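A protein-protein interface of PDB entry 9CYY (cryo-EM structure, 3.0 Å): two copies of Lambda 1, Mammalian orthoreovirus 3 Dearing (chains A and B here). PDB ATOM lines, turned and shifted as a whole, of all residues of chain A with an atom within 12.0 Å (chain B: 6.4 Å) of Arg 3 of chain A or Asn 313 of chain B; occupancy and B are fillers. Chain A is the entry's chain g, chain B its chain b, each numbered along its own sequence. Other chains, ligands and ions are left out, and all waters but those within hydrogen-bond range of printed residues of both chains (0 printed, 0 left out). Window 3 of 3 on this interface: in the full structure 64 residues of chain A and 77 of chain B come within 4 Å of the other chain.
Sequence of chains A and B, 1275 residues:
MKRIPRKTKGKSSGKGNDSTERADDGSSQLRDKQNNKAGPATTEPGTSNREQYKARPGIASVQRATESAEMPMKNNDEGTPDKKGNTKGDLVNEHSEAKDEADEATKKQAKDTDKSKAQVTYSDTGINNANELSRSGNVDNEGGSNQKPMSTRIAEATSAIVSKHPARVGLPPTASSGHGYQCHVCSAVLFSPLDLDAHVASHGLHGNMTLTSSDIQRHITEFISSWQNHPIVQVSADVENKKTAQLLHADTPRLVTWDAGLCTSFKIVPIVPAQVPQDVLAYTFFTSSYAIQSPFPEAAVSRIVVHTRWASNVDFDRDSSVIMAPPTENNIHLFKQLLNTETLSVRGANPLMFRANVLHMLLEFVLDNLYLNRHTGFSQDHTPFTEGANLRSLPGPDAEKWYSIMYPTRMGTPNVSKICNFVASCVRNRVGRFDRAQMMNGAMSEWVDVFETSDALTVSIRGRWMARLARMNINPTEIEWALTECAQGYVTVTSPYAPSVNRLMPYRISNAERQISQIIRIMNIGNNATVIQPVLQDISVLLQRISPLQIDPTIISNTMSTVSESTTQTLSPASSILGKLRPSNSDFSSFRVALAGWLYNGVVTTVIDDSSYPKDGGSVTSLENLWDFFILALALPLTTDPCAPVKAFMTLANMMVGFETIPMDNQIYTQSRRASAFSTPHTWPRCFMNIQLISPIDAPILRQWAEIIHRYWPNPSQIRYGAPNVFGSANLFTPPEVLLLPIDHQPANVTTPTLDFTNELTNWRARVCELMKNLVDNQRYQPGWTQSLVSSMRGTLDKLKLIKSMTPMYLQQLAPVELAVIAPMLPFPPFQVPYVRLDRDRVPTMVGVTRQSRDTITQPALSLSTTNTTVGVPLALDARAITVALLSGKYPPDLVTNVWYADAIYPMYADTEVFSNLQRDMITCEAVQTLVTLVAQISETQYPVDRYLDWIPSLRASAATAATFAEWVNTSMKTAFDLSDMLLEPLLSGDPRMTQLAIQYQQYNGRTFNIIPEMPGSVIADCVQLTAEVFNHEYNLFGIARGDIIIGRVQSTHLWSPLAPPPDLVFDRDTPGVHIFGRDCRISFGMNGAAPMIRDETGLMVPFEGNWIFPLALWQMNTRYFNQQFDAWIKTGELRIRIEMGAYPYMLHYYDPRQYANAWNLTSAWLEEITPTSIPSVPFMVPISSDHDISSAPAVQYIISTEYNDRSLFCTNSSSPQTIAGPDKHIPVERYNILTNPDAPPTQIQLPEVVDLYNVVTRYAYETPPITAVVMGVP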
ATOM      1  N   MET A   1      33.083 -16.914  -2.623  1.00  0.00           N
ATOM      2  CA  MET A   1      32.275 -18.127  -2.674  1.00  0.00           C
ATOM      3  C   MET A   1      31.096 -18.042  -1.714  1.00  0.00           C
ATOM      4  O   MET A   1      30.401 -19.032  -1.482  1.00  0.00           O
ATOM      5  CB  MET A   1      33.129 -19.354  -2.350  1.00  0.00           C
ATOM      6  CG  MET A   1      34.219 -19.650  -3.370  1.00  0.00           C
ATOM      7  SD  MET A   1      33.572 -20.006  -5.017  1.00  0.00           S
ATOM      8  CE  MET A   1      33.881 -18.452  -5.854  1.00  0.00           C
ATOM      9  N   LYS A   2      30.877 -16.856  -1.154  1.00  0.00           N
ATOM     10  CA  LYS A   2      29.766 -16.662  -0.237  1.00  0.00           C
ATOM     11  C   LYS A   2      28.436 -16.772  -0.976  1.00  0.00           C
ATOM     12  O   LYS A   2      28.313 -16.400  -2.145  1.00  0.00           O
ATOM     13  CB  LYS A   2      29.880 -15.305   0.459  1.00  0.00           C
ATOM     14  CG  LYS A   2      29.749 -14.110  -0.469  1.00  0.00           C
ATOM     15  CD  LYS A   2      29.836 -12.806   0.304  1.00  0.00           C
ATOM     16  CE  LYS A   2      31.255 -12.547   0.782  1.00  0.00           C
ATOM     17  NZ  LYS A   2      32.189 -12.316  -0.354  1.00  0.00           N
ATOM     18  N   ARG A   3      27.434 -17.299  -0.277  1.00  0.00           N
ATOM     19  CA  ARG A   3      26.111 -17.519  -0.847  1.00  0.00           C
ATOM     20  C   ARG A   3      25.289 -16.248  -0.668  1.00  0.00           C
ATOM     21  O   ARG A   3      24.907 -15.903   0.454  1.00  0.00           O
ATOM     22  CB  ARG A   3      25.431 -18.707  -0.172  1.00  0.00           C
ATOM     23  CG  ARG A   3      26.160 -20.031  -0.342  1.00  0.00           C
ATOM     24  CD  ARG A   3      26.124 -20.532  -1.773  1.00  0.00           C
ATOM     25  NE  ARG A   3      26.768 -21.835  -1.893  1.00  0.00           N
ATOM     26  CZ  ARG A   3      26.948 -22.485  -3.035  1.00  0.00           C
ATOM     27  NH1 ARG A   3      26.529 -21.986  -4.186  1.00  0.00           N
ATOM     28  NH2 ARG A   3      27.557 -23.665  -3.021  1.00  0.00           N
ATOM     29  N   ILE A   4      25.020 -15.551  -1.767  1.00  0.00           N
ATOM     30  CA  ILE A   4      24.222 -14.325  -1.662  1.00  0.00           C
ATOM     31  C   ILE A   4      22.753 -14.695  -1.493  1.00  0.00           C
ATOM     32  O   ILE A   4      22.191 -15.409  -2.346  1.00  0.00           O
ATOM     33  CB  ILE A   4      24.424 -13.439  -2.899  1.00  0.00           C
ATOM     34  CG1 ILE A   4      25.898 -13.068  -3.056  1.00  0.00           C
ATOM     35  CG2 ILE A   4      23.579 -12.187  -2.787  1.00  0.00           C
ATOM     36  CD1 ILE A   4      26.455 -12.283  -1.894  1.00  0.00           C
ATOM     37  N   PRO A   5      22.086 -14.253  -0.429  1.00  0.00           N
ATOM     38  CA  PRO A   5      20.671 -14.599  -0.246  1.00  0.00           C
ATOM     39  C   PRO A   5      19.769 -13.844  -1.211  1.00  0.00           C
ATOM     40  O   PRO A   5      20.079 -12.735  -1.649  1.00  0.00           O
ATOM     41  CB  PRO A   5      20.396 -14.192   1.205  1.00  0.00           C
ATOM     42  CG  PRO A   5      21.369 -13.097   1.469  1.00  0.00           C
ATOM     43  CD  PRO A   5      22.604 -13.428   0.674  1.00  0.00           C
ATOM     44  N   ARG A   6      18.639 -14.465  -1.538  1.00  0.00           N
ATOM     45  CA  ARG A   6      17.685 -13.858  -2.456  1.00  0.00           C
ATOM     46  C   ARG A   6      16.752 -12.904  -1.718  1.00  0.00           C
ATOM     47  O   ARG A   6      16.384 -13.139  -0.564  1.00  0.00           O
ATOM     48  CB  ARG A   6      16.868 -14.938  -3.163  1.00  0.00           C
ATOM     49  CG  ARG A   6      17.598 -15.635  -4.298  1.00  0.00           C
ATOM     50  CD  ARG A   6      16.654 -16.535  -5.076  1.00  0.00           C
ATOM     51  NE  ARG A   6      15.388 -15.873  -5.366  1.00  0.00           N
ATOM     52  CZ  ARG A   6      15.118 -15.236  -6.498  1.00  0.00           C
ATOM     53  NH1 ARG A   6      16.001 -15.169  -7.480  1.00  0.00           N
ATOM     54  NH2 ARG A   6      13.933 -14.655  -6.647  1.00  0.00           N
ATOM     55  N   LYS A   7      16.374 -11.815  -2.392  1.00  0.00           N
ATOM     56  CA  LYS A   7      15.378 -10.910  -1.831  1.00  0.00           C
ATOM     57  C   LYS A   7      13.999 -11.552  -1.773  1.00  0.00           C
ATOM     58  O   LYS A   7      13.326 -11.483  -0.738  1.00  0.00           O
ATOM     59  CB  LYS A   7      15.306  -9.622  -2.648  1.00  0.00           C
ATOM     60  CG  LYS A   7      16.518  -8.721  -2.542  1.00  0.00           C
ATOM     61  CD  LYS A   7      16.384  -7.555  -3.508  1.00  0.00           C
ATOM     62  CE  LYS A   7      15.302  -6.584  -3.060  1.00  0.00           C
ATOM     63  NZ  LYS A   7      15.234  -5.378  -3.932  1.00  0.00           N
ATOM     64  N   TRP B 258      28.200 -15.148 -10.684  1.00  0.00           N
ATOM     65  CA  TRP B 258      29.329 -16.007 -10.998  1.00  0.00           C
ATOM     66  C   TRP B 258      28.954 -17.474 -10.856  1.00  0.00           C
ATOM     67  O   TRP B 258      28.160 -17.853  -9.991  1.00  0.00           O
ATOM     68  CB  TRP B 258      30.524 -15.693 -10.098  1.00  0.00           C
ATOM     69  CG  TRP B 258      31.118 -14.355 -10.366  1.00  0.00           C
ATOM     70  CD1 TRP B 258      30.852 -13.193  -9.707  1.00  0.00           C
ATOM     71  CD2 TRP B 258      32.072 -14.032 -11.381  1.00  0.00           C
ATOM     72  NE1 TRP B 258      31.587 -12.166 -10.245  1.00  0.00           N
ATOM     73  CE2 TRP B 258      32.345 -12.656 -11.274  1.00  0.00           C
ATOM     74  CE3 TRP B 258      32.725 -14.775 -12.367  1.00  0.00           C
ATOM     75  CZ2 TRP B 258      33.241 -12.008 -12.116  1.00  0.00           C
ATOM     76  CZ3 TRP B 258      33.614 -14.130 -13.200  1.00  0.00           C
ATOM     77  CH2 TRP B 258      33.864 -12.761 -13.070  1.00  0.00           C
ATOM     78  N   ASP B 259      29.542 -18.295 -11.723  1.00  0.00           N
ATOM     79  CA  ASP B 259      29.380 -19.741 -11.691  1.00  0.00           C
ATOM     80  C   ASP B 259      30.754 -20.387 -11.755  1.00  0.00           C
ATOM     81  O   ASP B 259      31.567 -20.038 -12.616  1.00  0.00           O
ATOM     82  CB  ASP B 259      28.514 -20.231 -12.851  1.00  0.00           C
ATOM     83  CG  ASP B 259      28.416 -21.738 -12.906  1.00  0.00           C
ATOM     84  OD1 ASP B 259      27.699 -22.318 -12.067  1.00  0.00           O
ATOM     85  OD2 ASP B 259      29.061 -22.346 -13.785  1.00  0.00           O
ATOM     86  N   ALA B 260      31.010 -21.330 -10.849  1.00  0.00           N
ATOM     87  CA  ALA B 260      32.305 -21.995 -10.769  1.00  0.00           C
ATOM     88  C   ALA B 260      32.200 -23.495 -11.012  1.00  0.00           C
ATOM     89  O   ALA B 260      33.115 -24.240 -10.657  1.00  0.00           O
ATOM     90  CB  ALA B 260      32.960 -21.725  -9.414  1.00  0.00           C
ATOM     91  N   GLY B 261      31.109 -23.950 -11.609  1.00  0.00           N
ATOM     92  CA  GLY B 261      30.897 -25.359 -11.898  1.00  0.00           C
ATOM     93  C   GLY B 261      31.219 -25.700 -13.336  1.00  0.00           C
ATOM     94  O   GLY B 261      32.222 -25.244 -13.894  1.00  0.00           O
ATOM     95  N   LEU B 262      30.361 -26.514 -13.943  1.00  0.00           N
ATOM     96  CA  LEU B 262      30.496 -26.893 -15.341  1.00  0.00           C
ATOM     97  C   LEU B 262      29.488 -26.126 -16.185  1.00  0.00           C
ATOM     98  O   LEU B 262      28.387 -25.812 -15.725  1.00  0.00           O
ATOM     99  CB  LEU B 262      30.295 -28.397 -15.525  1.00  0.00           C
ATOM    100  CG  LEU B 262      31.315 -29.311 -14.848  1.00  0.00           C
ATOM    101  CD1 LEU B 262      30.917 -30.766 -15.020  1.00  0.00           C
ATOM    102  CD2 LEU B 262      32.706 -29.068 -15.402  1.00  0.00           C
ATOM    103  N   ALA B 311      25.292 -29.323 -12.589  1.00  0.00           N
ATOM    104  CA  ALA B 311      26.624 -29.472 -12.018  1.00  0.00           C
ATOM    105  C   ALA B 311      27.224 -28.072 -11.868  1.00  0.00           C
ATOM    106  O   ALA B 311      28.380 -27.808 -12.192  1.00  0.00           O
ATOM    107  CB  ALA B 311      27.511 -30.377 -12.874  1.00  0.00           C
ATOM    108  N   SER B 312      26.418 -27.145 -11.357  1.00  0.00           N
ATOM    109  CA  SER B 312      26.805 -25.744 -11.279  1.00  0.00           C
ATOM    110  C   SER B 312      26.975 -25.333  -9.828  1.00  0.00           C
ATOM    111  O   SER B 312      26.164 -25.705  -8.974  1.00  0.00           O
ATOM    112  CB  SER B 312      25.761 -24.847 -11.950  1.00  0.00           C
ATOM    113  OG  SER B 312      24.630 -24.692 -11.114  1.00  0.00           O
ATOM    114  N   ASN B 313      28.027 -24.568  -9.555  1.00  0.00           N
ATOM    115  CA  ASN B 313      28.268 -23.986  -8.239  1.00  0.00           C
ATOM    116  C   ASN B 313      28.239 -22.469  -8.390  1.00  0.00           C
ATOM    117  O   ASN B 313      29.143 -21.883  -8.992  1.00  0.00           O
ATOM    118  CB  ASN B 313      29.601 -24.464  -7.673  1.00  0.00           C
ATOM    119  CG  ASN B 313      29.755 -24.153  -6.202  1.00  0.00           C
ATOM    120  OD1 ASN B 313      28.896 -23.514  -5.598  1.00  0.00           O
ATOM    121  ND2 ASN B 313      30.854 -24.607  -5.614  1.00  0.00           N
ATOM    122  N   VAL B 314      27.204 -21.836  -7.842  1.00  0.00           N
ATOM    123  CA  VAL B 314      26.969 -20.414  -8.047  1.00  0.00           C
ATOM    124  C   VAL B 314      26.992 -19.700  -6.704  1.00  0.00           C
ATOM    125  O   VAL B 314      26.940 -20.319  -5.639  1.00  0.00           O
ATOM    126  CB  VAL B 314      25.635 -20.145  -8.770  1.00  0.00           C
ATOM    127  CG1 VAL B 314      25.581 -20.897 -10.085  1.00  0.00           C
ATOM    128  CG2 VAL B 314      24.468 -20.527  -7.881  1.00  0.00           C
ATOM    129  N   ASP B 315      27.076 -18.373  -6.769  1.00  0.00           N
ATOM    130  CA  ASP B 315      26.990 -17.544  -5.574  1.00  0.00           C
ATOM    131  C   ASP B 315      25.596 -16.956  -5.388  1.00  0.00           C
ATOM    132  O   ASP B 315      25.169 -16.722  -4.254  1.00  0.00           O
ATOM    133  CB  ASP B 315      28.030 -16.422  -5.634  1.00  0.00           C
ATOM    134  CG  ASP B 315      27.767 -15.443  -6.758  1.00  0.00           C
ATOM    135  OD1 ASP B 315      27.159 -15.847  -7.770  1.00  0.00           O
ATOM    136  OD2 ASP B 315      28.168 -14.267  -6.631  1.00  0.00           O
ATOM    137  N   PHE B 316      24.884 -16.710  -6.485  1.00  0.00           N
ATOM    138  CA  PHE B 316      23.509 -16.240  -6.452  1.00  0.00           C
ATOM    139  C   PHE B 316      22.674 -17.134  -7.354  1.00  0.00           C
ATOM    140  O   PHE B 316      23.099 -17.485  -8.458  1.00  0.00           O
ATOM    141  CB  PHE B 316      23.413 -14.774  -6.900  1.00  0.00           C
ATOM    142  CG  PHE B 316      22.007 -14.261  -7.018  1.00  0.00           C
ATOM    143  CD1 PHE B 316      21.373 -13.693  -5.929  1.00  0.00           C
ATOM    144  CD2 PHE B 316      21.323 -14.336  -8.219  1.00  0.00           C
ATOM    145  CE1 PHE B 316      20.083 -13.215  -6.033  1.00  0.00           C
ATOM    146  CE2 PHE B 316      20.033 -13.861  -8.327  1.00  0.00           C
ATOM    147  CZ  PHE B 316      19.413 -13.300  -7.233  1.00  0.00           C
ATOM    148  N   LEU B 394      37.581 -28.492  -9.244  1.00  0.00           N
ATOM    149  CA  LEU B 394      36.339 -27.877  -8.811  1.00  0.00           C
ATOM    150  C   LEU B 394      36.420 -27.549  -7.320  1.00  0.00           C
ATOM    151  O   LEU B 394      37.075 -28.263  -6.556  1.00  0.00           O
ATOM    152  CB  LEU B 394      35.166 -28.815  -9.087  1.00  0.00           C
ATOM    153  CG  LEU B 394      34.468 -28.650 -10.441  1.00  0.00           C
ATOM    154  CD1 LEU B 394      33.476 -29.773 -10.675  1.00  0.00           C
ATOM    155  CD2 LEU B 394      33.780 -27.310 -10.558  1.00  0.00           C
ATOM    156  N   PRO B 395      35.771 -26.473  -6.875  1.00  0.00           N
ATOM    157  CA  PRO B 395      35.839 -26.122  -5.452  1.00  0.00           C
ATOM    158  C   PRO B 395      35.042 -27.100  -4.602  1.00  0.00           C
ATOM    159  O   PRO B 395      34.082 -27.718  -5.064  1.00  0.00           O
ATOM    160  CB  PRO B 395      35.247 -24.710  -5.399  1.00  0.00           C
ATOM    161  CG  PRO B 395      34.460 -24.548  -6.648  1.00  0.00           C
ATOM    162  CD  PRO B 395      34.796 -25.649  -7.608  1.00  0.00           C
ATOM    163  N   GLY B 396      35.454 -27.234  -3.344  1.00  0.00           N
ATOM    164  CA  GLY B 396      34.811 -28.136  -2.422  1.00  0.00           C
ATOM    165  C   GLY B 396      35.542 -29.459  -2.318  1.00  0.00           C
ATOM    166  O   GLY B 396      36.673 -29.608  -2.790  1.00  0.00           O
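The guanidinium group (NH1) of Arg 3 of chain A sits close to the backbone carbonyl oxygen (O) of Val 314 of chain B, 2.2 Å away.
OD1 of Asn 313 of chain B lies within hydrogen-bond range of NH2 of Arg 3 of chain A (2.9 Å).
N of Ile 4 of chain A lies within hydrogen-bond range of O of Asp 315 of chain B.
N of Trp 258 of chain B is in hydrogen-bond range of OD1 of Asp 315 of chain B (3.2 Å).
The side-chain carboxylate (OD1) of Asp 259 of chain B lies within hydrogen-bond range of the backbone NH (N) of Asn 313 of chain B.
N of Ala 260 of chain B sits at hydrogen-bond distance from O of Asn 313 of chain B (2.7 Å).
CB of Asp 315 of chain B touches O of Lys 2 of chain A (3.5 Å).
Arg 3 of chain A touches Asp 315 of chain B.
Phe 316 of chain B touches Arg 6 of chain A (CE1 to CG, 3.9 Å).
Of chain B, only Asn 313 (2.9 Å), Val 314 (2.2 Å) and Asp 315 (3.6 Å) come within 4 Å of Arg 3 of chain A.
Of the printed residues of chain B, Ile 4 of chain A touches Asp 315.
Printed residues of chain B within 4 Å of Arg 6 of chain A: Phe 316 (3.9 Å).
Lys 7 of chain A touches none of the printed residues of chain B.
No residue of chain A comes within 4 Å of Asp 259 of chain B.
No residue of chain A comes within 4 Å of Ala 260 of chain B.
No residue of chain A comes within 4 Å of Gly 261 of chain B.
No residue of chain A comes within 4 Å of Ala 311 of chain B.
No residue of chain A comes within 4 Å of Ser 312 of chain B.
Asn 313 of chain B touches just one residue of chain A: Arg 3.
No residue of chain A comes within 4 Å of Pro 395 of chain B.
Hydrophobic or aromatic side chains of chain B within 4 Å of the printed part of chain A: Phe 316.
Of the 7 printed residues of chain A, 4 touch a printed residue of chain B.
Hydrophobic or aromatic side chains of chain A within 4 Å of the printed part of chain B: Ile 4.
Along chain A the printed residues that touch a printed residue of chain B span positions 2 to 6.
Among the printed residues, 6 pairs touch across the chains.
No position is printed for both chains.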
